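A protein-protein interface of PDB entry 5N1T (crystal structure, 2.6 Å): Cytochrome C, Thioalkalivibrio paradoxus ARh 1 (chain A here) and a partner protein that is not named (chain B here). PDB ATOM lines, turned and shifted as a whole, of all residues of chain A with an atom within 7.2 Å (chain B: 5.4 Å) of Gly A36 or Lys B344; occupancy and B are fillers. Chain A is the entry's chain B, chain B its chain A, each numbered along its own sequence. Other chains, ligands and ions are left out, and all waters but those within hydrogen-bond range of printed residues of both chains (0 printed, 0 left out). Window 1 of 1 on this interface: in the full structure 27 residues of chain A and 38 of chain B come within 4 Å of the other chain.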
ATOM      1  N   ARG A  30      -1.878 -11.765   2.154  1.00  0.00           N
ATOM      2  CA  ARG A  30      -3.217 -12.070   1.672  1.00  0.00           C
ATOM      3  C   ARG A  30      -3.545 -11.347   0.364  1.00  0.00           C
ATOM      4  O   ARG A  30      -3.906 -11.995  -0.619  1.00  0.00           O
ATOM      5  CB  ARG A  30      -4.280 -11.789   2.728  1.00  0.00           C
ATOM      6  CG  ARG A  30      -5.703 -12.011   2.245  1.00  0.00           C
ATOM      7  CD  ARG A  30      -5.963 -13.475   1.998  1.00  0.00           C
ATOM      8  NE  ARG A  30      -7.331 -13.664   1.533  1.00  0.00           N
ATOM      9  CZ  ARG A  30      -7.740 -14.596   0.670  1.00  0.00           C
ATOM     10  NH1 ARG A  30      -6.888 -15.461   0.130  1.00  0.00           N
ATOM     11  NH2 ARG A  30      -9.024 -14.647   0.333  1.00  0.00           N
ATOM     12  N   GLY A  31      -3.396 -10.025   0.334  1.00  0.00           N
ATOM     13  CA  GLY A  31      -3.736  -9.258  -0.863  1.00  0.00           C
ATOM     14  C   GLY A  31      -2.777  -9.562  -1.992  1.00  0.00           C
ATOM     15  O   GLY A  31      -3.153  -9.591  -3.174  1.00  0.00           O
ATOM     16  N   ALA A  32      -1.522  -9.791  -1.627  1.00  0.00           N
ATOM     17  CA  ALA A  32      -0.480 -10.074  -2.594  1.00  0.00           C
ATOM     18  C   ALA A  32      -0.764 -11.380  -3.361  1.00  0.00           C
ATOM     19  O   ALA A  32      -0.547 -11.451  -4.560  1.00  0.00           O
ATOM     20  CB  ALA A  32       0.873 -10.113  -1.899  1.00  0.00           C
ATOM     21  N   LEU A  33      -1.284 -12.382  -2.654  1.00  0.00           N
ATOM     22  CA  LEU A  33      -1.601 -13.683  -3.240  1.00  0.00           C
ATOM     23  C   LEU A  33      -2.831 -13.609  -4.105  1.00  0.00           C
ATOM     24  O   LEU A  33      -2.849 -14.234  -5.172  1.00  0.00           O
ATOM     25  CB  LEU A  33      -1.758 -14.772  -2.171  1.00  0.00           C
ATOM     26  CG  LEU A  33      -0.483 -15.095  -1.395  1.00  0.00           C
ATOM     27  CD1 LEU A  33      -0.726 -16.127  -0.294  1.00  0.00           C
ATOM     28  CD2 LEU A  33       0.633 -15.545  -2.335  1.00  0.00           C
ATOM     29  N   LEU A  34      -3.829 -12.831  -3.664  1.00  0.00           N
ATOM     30  CA  LEU A  34      -5.070 -12.604  -4.422  1.00  0.00           C
ATOM     31  C   LEU A  34      -4.755 -11.924  -5.724  1.00  0.00           C
ATOM     32  O   LEU A  34      -5.341 -12.271  -6.758  1.00  0.00           O
ATOM     33  CB  LEU A  34      -6.095 -11.789  -3.639  1.00  0.00           C
ATOM     34  CG  LEU A  34      -6.781 -12.492  -2.465  1.00  0.00           C
ATOM     35  CD1 LEU A  34      -7.474 -11.444  -1.622  1.00  0.00           C
ATOM     36  CD2 LEU A  34      -7.768 -13.593  -2.863  1.00  0.00           C
ATOM     37  N   ALA A  35      -3.789 -11.002  -5.670  1.00  0.00           N
ATOM     38  CA  ALA A  35      -3.425 -10.171  -6.809  1.00  0.00           C
ATOM     39  C   ALA A  35      -2.385 -10.815  -7.735  1.00  0.00           C
ATOM     40  O   ALA A  35      -2.491 -10.696  -8.963  1.00  0.00           O
ATOM     41  CB  ALA A  35      -2.939  -8.821  -6.311  1.00  0.00           C
ATOM     42  N   GLY A  36      -1.396 -11.502  -7.151  1.00  0.00           N
ATOM     43  CA  GLY A  36      -0.261 -12.113  -7.886  1.00  0.00           C
ATOM     44  C   GLY A  36      -0.608 -12.868  -9.173  1.00  0.00           C
ATOM     45  O   GLY A  36       0.124 -12.781 -10.193  1.00  0.00           O
ATOM     46  N   ASN A  37      -1.742 -13.580  -9.116  1.00  0.00           N
ATOM     47  CA  ASN A  37      -2.213 -14.395 -10.208  1.00  0.00           C
ATOM     48  C   ASN A  37      -2.618 -13.573 -11.426  1.00  0.00           C
ATOM     49  O   ASN A  37      -2.489 -14.026 -12.567  1.00  0.00           O
ATOM     50  CB  ASN A  37      -3.322 -15.326  -9.710  1.00  0.00           C
ATOM     51  CG  ASN A  37      -2.771 -16.503  -8.901  1.00  0.00           C
ATOM     52  OD1 ASN A  37      -2.004 -17.315  -9.415  1.00  0.00           O
ATOM     53  ND2 ASN A  37      -3.166 -16.601  -7.640  1.00  0.00           N
ATOM     54  N   CYS A  38      -3.058 -12.349 -11.193  1.00  0.00           N
ATOM     55  CA  CYS A  38      -3.402 -11.437 -12.290  1.00  0.00           C
ATOM     56  C   CYS A  38      -2.204 -11.138 -13.147  1.00  0.00           C
ATOM     57  O   CYS A  38      -2.343 -10.938 -14.351  1.00  0.00           O
ATOM     58  CB  CYS A  38      -3.964 -10.119 -11.756  1.00  0.00           C
ATOM     59  SG  CYS A  38      -5.232 -10.364 -10.502  1.00  0.00           S
ATOM     60  N   TYR A  39      -1.023 -11.118 -12.535  1.00  0.00           N
ATOM     61  CA  TYR A  39       0.181 -10.829 -13.296  1.00  0.00           C
ATOM     62  C   TYR A  39       0.517 -11.982 -14.226  1.00  0.00           C
ATOM     63  O   TYR A  39       1.160 -11.775 -15.247  1.00  0.00           O
ATOM     64  CB  TYR A  39       1.368 -10.432 -12.401  1.00  0.00           C
ATOM     65  CG  TYR A  39       1.069  -9.331 -11.366  1.00  0.00           C
ATOM     66  CD1 TYR A  39       0.384  -8.162 -11.724  1.00  0.00           C
ATOM     67  CD2 TYR A  39       1.496  -9.460 -10.017  1.00  0.00           C
ATOM     68  CE1 TYR A  39       0.110  -7.178 -10.781  1.00  0.00           C
ATOM     69  CE2 TYR A  39       1.232  -8.465  -9.073  1.00  0.00           C
ATOM     70  CZ  TYR A  39       0.537  -7.324  -9.461  1.00  0.00           C
ATOM     71  OH  TYR A  39       0.253  -6.318  -8.540  1.00  0.00           O
ATOM     72  N   GLY A  40       0.056 -13.183 -13.868  1.00  0.00           N
ATOM     73  CA  GLY A  40       0.199 -14.384 -14.682  1.00  0.00           C
ATOM     74  C   GLY A  40      -0.216 -14.171 -16.124  1.00  0.00           C
ATOM     75  O   GLY A  40       0.531 -14.551 -17.029  1.00  0.00           O
ATOM     76  N   CYS A  41      -1.378 -13.550 -16.348  1.00  0.00           N
ATOM     77  CA  CYS A  41      -1.795 -13.137 -17.713  1.00  0.00           C
ATOM     78  C   CYS A  41      -1.482 -11.689 -18.046  1.00  0.00           C
ATOM     79  O   CYS A  41      -1.207 -11.383 -19.213  1.00  0.00           O
ATOM     80  CB  CYS A  41      -3.292 -13.265 -17.947  1.00  0.00           C
ATOM     81  SG  CYS A  41      -4.045 -14.902 -17.952  1.00  0.00           S
ATOM     82  N   GLY A  43       0.903  -9.667 -17.022  1.00  0.00           N
ATOM     83  CA  GLY A  43       2.332  -9.292 -17.115  1.00  0.00           C
ATOM     84  C   GLY A  43       2.856  -8.840 -15.777  1.00  0.00           C
ATOM     85  O   GLY A  43       2.042  -8.577 -14.899  1.00  0.00           O
ATOM     86  N   ILE A  95      -7.821  -6.986  -4.232  1.00  0.00           N
ATOM     87  CA  ILE A  95      -7.084  -7.134  -5.491  1.00  0.00           C
ATOM     88  C   ILE A  95      -6.949  -5.765  -6.150  1.00  0.00           C
ATOM     89  O   ILE A  95      -5.849  -5.368  -6.589  1.00  0.00           O
ATOM     90  CB  ILE A  95      -7.798  -8.142  -6.435  1.00  0.00           C
ATOM     91  CG1 ILE A  95      -7.604  -9.552  -5.935  1.00  0.00           C
ATOM     92  CG2 ILE A  95      -7.301  -8.073  -7.878  1.00  0.00           C
ATOM     93  CD1 ILE A  95      -8.788 -10.429  -6.270  1.00  0.00           C
ATOM     94  N   HIS A  98      -4.460  -3.403  -4.074  1.00  0.00           N
ATOM     95  CA  HIS A  98      -3.096  -3.893  -4.222  1.00  0.00           C
ATOM     96  C   HIS A  98      -2.453  -3.666  -5.610  1.00  0.00           C
ATOM     97  O   HIS A  98      -1.276  -3.281  -5.685  1.00  0.00           O
ATOM     98  CB  HIS A  98      -3.028  -5.363  -3.793  1.00  0.00           C
ATOM     99  CG  HIS A  98      -1.637  -5.892  -3.671  1.00  0.00           C
ATOM    100  ND1 HIS A  98      -1.027  -6.097  -2.449  1.00  0.00           N
ATOM    101  CD2 HIS A  98      -0.736  -6.265  -4.621  1.00  0.00           C
ATOM    102  CE1 HIS A  98       0.194  -6.571  -2.656  1.00  0.00           C
ATOM    103  NE2 HIS A  98       0.397  -6.677  -3.964  1.00  0.00           N
ATOM    104  N   ILE A  99      -3.203  -3.859  -6.693  1.00  0.00           N
ATOM    105  CA  ILE A  99      -2.627  -3.622  -8.027  1.00  0.00           C
ATOM    106  C   ILE A  99      -2.334  -2.134  -8.272  1.00  0.00           C
ATOM    107  O   ILE A  99      -1.223  -1.791  -8.673  1.00  0.00           O
ATOM    108  CB  ILE A  99      -3.416  -4.319  -9.167  1.00  0.00           C
ATOM    109  CG1 ILE A  99      -3.215  -5.835  -9.070  1.00  0.00           C
ATOM    110  CG2 ILE A  99      -2.953  -3.853 -10.537  1.00  0.00           C
ATOM    111  CD1 ILE A  99      -4.356  -6.632  -9.663  1.00  0.00           C
ATOM    112  N   THR B  51       9.592 -18.555 -10.767  1.00  0.00           N
ATOM    113  CA  THR B  51       8.562 -17.776 -10.080  1.00  0.00           C
ATOM    114  C   THR B  51       8.799 -17.747  -8.544  1.00  0.00           C
ATOM    115  O   THR B  51       8.712 -16.683  -7.933  1.00  0.00           O
ATOM    116  CB  THR B  51       7.123 -18.234 -10.439  1.00  0.00           C
ATOM    117  OG1 THR B  51       7.003 -18.343 -11.858  1.00  0.00           O
ATOM    118  CG2 THR B  51       6.074 -17.240  -9.936  1.00  0.00           C
ATOM    119  N   TYR B  55       9.754 -14.314  -6.294  1.00  0.00           N
ATOM    120  CA  TYR B  55       8.773 -13.864  -5.310  1.00  0.00           C
ATOM    121  C   TYR B  55       9.316 -13.891  -3.900  1.00  0.00           C
ATOM    122  O   TYR B  55       8.879 -13.110  -3.032  1.00  0.00           O
ATOM    123  CB  TYR B  55       7.450 -14.655  -5.420  1.00  0.00           C
ATOM    124  CG  TYR B  55       6.414 -13.984  -6.315  1.00  0.00           C
ATOM    125  CD1 TYR B  55       6.620 -13.893  -7.706  1.00  0.00           C
ATOM    126  CD2 TYR B  55       5.258 -13.408  -5.777  1.00  0.00           C
ATOM    127  CE1 TYR B  55       5.698 -13.280  -8.520  1.00  0.00           C
ATOM    128  CE2 TYR B  55       4.317 -12.792  -6.593  1.00  0.00           C
ATOM    129  CZ  TYR B  55       4.545 -12.745  -7.959  1.00  0.00           C
ATOM    130  OH  TYR B  55       3.637 -12.151  -8.812  1.00  0.00           O
ATOM    131  N   PHE B  59       9.139 -10.894  -1.467  1.00  0.00           N
ATOM    132  CA  PHE B  59       8.487 -10.969  -0.181  1.00  0.00           C
ATOM    133  C   PHE B  59       9.422 -10.703   0.985  1.00  0.00           C
ATOM    134  O   PHE B  59       9.015 -10.148   2.002  1.00  0.00           O
ATOM    135  CB  PHE B  59       7.803 -12.306  -0.034  1.00  0.00           C
ATOM    136  CG  PHE B  59       6.489 -12.378  -0.741  1.00  0.00           C
ATOM    137  CD1 PHE B  59       5.791 -11.212  -1.070  1.00  0.00           C
ATOM    138  CD2 PHE B  59       5.922 -13.608  -1.055  1.00  0.00           C
ATOM    139  CE1 PHE B  59       4.550 -11.275  -1.719  1.00  0.00           C
ATOM    140  CE2 PHE B  59       4.690 -13.670  -1.706  1.00  0.00           C
ATOM    141  CZ  PHE B  59       3.996 -12.503  -2.037  1.00  0.00           C
ATOM    142  N   ALA B 339       1.883 -24.219 -11.665  1.00  0.00           N
ATOM    143  CA  ALA B 339       3.216 -24.158 -11.055  1.00  0.00           C
ATOM    144  C   ALA B 339       3.554 -22.716 -10.592  1.00  0.00           C
ATOM    145  O   ALA B 339       3.877 -22.497  -9.427  1.00  0.00           O
ATOM    146  CB  ALA B 339       4.263 -24.668 -12.029  1.00  0.00           C
ATOM    147  N   ASN B 340       3.402 -21.746 -11.503  1.00  0.00           N
ATOM    148  CA  ASN B 340       3.678 -20.347 -11.258  1.00  0.00           C
ATOM    149  C   ASN B 340       2.806 -19.835 -10.115  1.00  0.00           C
ATOM    150  O   ASN B 340       3.263 -19.071  -9.234  1.00  0.00           O
ATOM    151  CB  ASN B 340       3.443 -19.565 -12.535  1.00  0.00           C
ATOM    152  CG  ASN B 340       3.326 -18.061 -12.304  1.00  0.00           C
ATOM    153  OD1 ASN B 340       2.315 -17.556 -11.766  1.00  0.00           O
ATOM    154  ND2 ASN B 340       4.338 -17.327 -12.756  1.00  0.00           N
ATOM    155  N   SER B 341       1.557 -20.288 -10.121  1.00  0.00           N
ATOM    156  CA  SER B 341       0.613 -19.866  -9.118  1.00  0.00           C
ATOM    157  C   SER B 341       1.050 -20.413  -7.789  1.00  0.00           C
ATOM    158  O   SER B 341       1.139 -19.656  -6.834  1.00  0.00           O
ATOM    159  CB  SER B 341      -0.775 -20.313  -9.489  1.00  0.00           C
ATOM    160  OG  SER B 341      -1.733 -19.735  -8.637  1.00  0.00           O
ATOM    161  N   GLN B 342       1.400 -21.702  -7.761  1.00  0.00           N
ATOM    162  CA  GLN B 342       1.775 -22.418  -6.535  1.00  0.00           C
ATOM    163  C   GLN B 342       3.027 -21.809  -5.923  1.00  0.00           C
ATOM    164  O   GLN B 342       3.183 -21.791  -4.711  1.00  0.00           O
ATOM    165  CB  GLN B 342       2.040 -23.891  -6.827  1.00  0.00           C
ATOM    166  CG  GLN B 342       0.796 -24.738  -7.023  1.00  0.00           C
ATOM    167  CD  GLN B 342       1.017 -25.888  -7.992  1.00  0.00           C
ATOM    168  OE1 GLN B 342       2.134 -26.069  -8.491  1.00  0.00           O
ATOM    169  NE2 GLN B 342      -0.062 -26.671  -8.287  1.00  0.00           N
ATOM    170  N   ALA B 343       3.886 -21.292  -6.796  1.00  0.00           N
ATOM    171  CA  ALA B 343       5.169 -20.697  -6.445  1.00  0.00           C
ATOM    172  C   ALA B 343       5.004 -19.507  -5.535  1.00  0.00           C
ATOM    173  O   ALA B 343       5.776 -19.369  -4.602  1.00  0.00           O
ATOM    174  CB  ALA B 343       5.878 -20.256  -7.704  1.00  0.00           C
ATOM    175  N   LYS B 344       4.019 -18.651  -5.856  1.00  0.00           N
ATOM    176  CA  LYS B 344       3.686 -17.412  -5.127  1.00  0.00           C
ATOM    177  C   LYS B 344       3.227 -17.708  -3.706  1.00  0.00           C
ATOM    178  O   LYS B 344       3.900 -17.255  -2.767  1.00  0.00           O
ATOM    179  CB  LYS B 344       2.664 -16.557  -5.885  1.00  0.00           C
ATOM    180  CG  LYS B 344       3.200 -16.109  -7.248  1.00  0.00           C
ATOM    181  CD  LYS B 344       2.124 -15.836  -8.296  1.00  0.00           C
ATOM    182  CE  LYS B 344       2.824 -15.283  -9.523  1.00  0.00           C
ATOM    183  NZ  LYS B 344       1.854 -14.794 -10.535  1.00  0.00           N
ATOM    184  N   VAL B 345       2.131 -18.476  -3.560  1.00  0.00           N
ATOM    185  CA  VAL B 345       1.674 -19.028  -2.271  1.00  0.00           C
ATOM    186  C   VAL B 345       2.844 -19.595  -1.484  1.00  0.00           C
ATOM    187  O   VAL B 345       2.997 -19.249  -0.306  1.00  0.00           O
ATOM    188  CB  VAL B 345       0.542 -20.091  -2.451  1.00  0.00           C
ATOM    189  CG1 VAL B 345       0.354 -20.976  -1.217  1.00  0.00           C
ATOM    190  CG2 VAL B 345      -0.763 -19.416  -2.828  1.00  0.00           C
ATOM    191  N   CYS B 346       3.689 -20.387  -2.155  1.00  0.00           N
ATOM    192  CA  CYS B 346       4.864 -21.046  -1.536  1.00  0.00           C
ATOM    193  C   CYS B 346       5.892 -20.073  -0.988  1.00  0.00           C
ATOM    194  O   CYS B 346       6.357 -20.265   0.119  1.00  0.00           O
ATOM    195  CB  CYS B 346       5.569 -22.029  -2.489  1.00  0.00           C
ATOM    196  SG  CYS B 346       6.936 -23.015  -1.781  1.00  0.00           S
ATOM    197  N   ALA B 347       6.241 -19.050  -1.761  1.00  0.00           N
ATOM    198  CA  ALA B 347       7.180 -17.991  -1.347  1.00  0.00           C
ATOM    199  C   ALA B 347       6.671 -17.325  -0.080  1.00  0.00           C
ATOM    200  O   ALA B 347       7.354 -17.327   0.945  1.00  0.00           O
ATOM    201  CB  ALA B 347       7.369 -16.964  -2.462  1.00  0.00           C
ATOM    202  N   ALA B 348       5.439 -16.837  -0.143  1.00  0.00           N
ATOM    203  CA  ALA B 348       4.747 -16.299   1.009  1.00  0.00           C
ATOM    204  C   ALA B 348       4.795 -17.237   2.222  1.00  0.00           C
ATOM    205  O   ALA B 348       5.028 -16.791   3.336  1.00  0.00           O
ATOM    206  CB  ALA B 348       3.314 -15.977   0.637  1.00  0.00           C
ATOM    207  N   ALA B 349       4.594 -18.533   1.995  1.00  0.00           N
ATOM    208  CA  ALA B 349       4.520 -19.470   3.090  1.00  0.00           C
ATOM    209  C   ALA B 349       5.877 -19.708   3.718  1.00  0.00           C
ATOM    210  O   ALA B 349       5.924 -19.980   4.930  1.00  0.00           O
ATOM    211  CB  ALA B 349       3.930 -20.781   2.625  1.00  0.00           C
ATOM    212  N   GLU B 426       7.166 -12.397 -16.537  1.00  0.00           N
ATOM    213  CA  GLU B 426       7.135 -12.466 -15.101  1.00  0.00           C
ATOM    214  C   GLU B 426       8.267 -13.361 -14.570  1.00  0.00           C
ATOM    215  O   GLU B 426       8.982 -12.966 -13.654  1.00  0.00           O
ATOM    216  CB  GLU B 426       5.768 -12.905 -14.579  1.00  0.00           C
ATOM    217  CG  GLU B 426       5.688 -12.756 -13.064  1.00  0.00           C
ATOM    218  CD  GLU B 426       4.369 -13.164 -12.435  1.00  0.00           C
ATOM    219  OE1 GLU B 426       3.835 -14.257 -12.782  1.00  0.00           O
ATOM    220  OE2 GLU B 426       3.899 -12.376 -11.544  1.00  0.00           O
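Among the printed residues, merely in contact across the chains: Tyr A39 with Glu B426, Leu A33 with Val B345, Tyr A39 with Tyr B55, Leu A33 with Lys B344, Gly A36 with Tyr B55 and Ala A32 with Phe B59.
Of chain B, only Tyr B55 (3.8 Å) and Lys B344 (2.7 Å) come within 4 Å of Gly A36.
Lys B344 touches two residues of chain A.
No residue of chain A comes within 4 Å of Ala B343.
Printed residues of chain A within 4 Å of Val B345: Leu A33.
Of the printed residues of chain B, Ala A32 touches Phe B59 (3.9 Å).
Of the printed residues of chain B, Leu A33 touches Lys B344 (3.6 Å) and Val B345 (3.5 Å).
The nearest residue of chain B that does not touch Gly A36 is Glu B426 (4.03 Å).
The nearest residue of chain A that does not touch Lys B344 is Asn A37 (4.1 Å).
Of the 15 printed residues of chain B, 6 touch a printed residue of chain A.
Hydrophobic or aromatic side chains of chain B that line the printed part of chain A: Tyr B55 and Phe B59.
Among the printed residues, no Asp or Glu carboxylate lies within 4 Å of a Lys or Arg side-chain nitrogen of the other chain.
ND2 of Asn B340 lies within hydrogen-bond range of OE1 of Glu B426 (3.1 Å).
The side-chain amino group of Lys B344 lies within hydrogen-bond range of the side-chain amide oxygen of Asn B340, 3.1 Å away.
The side-chain hydroxyl (OH) of Tyr B55 sits at hydrogen-bond distance from the side-chain carboxylate (OE2) of Glu B426.
NZ of Lys B344 is in salt-bridge range of OE1 of Glu B426 (3.0 Å).
The side-chain amide nitrogen (ND2) of Asn A37 lies within hydrogen-bond range of the backbone carbonyl oxygen (O) of Leu A33 (3.4 Å).
The side-chain hydroxyl of Ser B341 sits at hydrogen-bond distance from the side-chain amide oxygen of Asn A37, at 2.6 Å.
The side-chain amino group of Lys B344 is in hydrogen-bond range of the backbone carbonyl oxygen of Gly A36 (2.7 Å).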
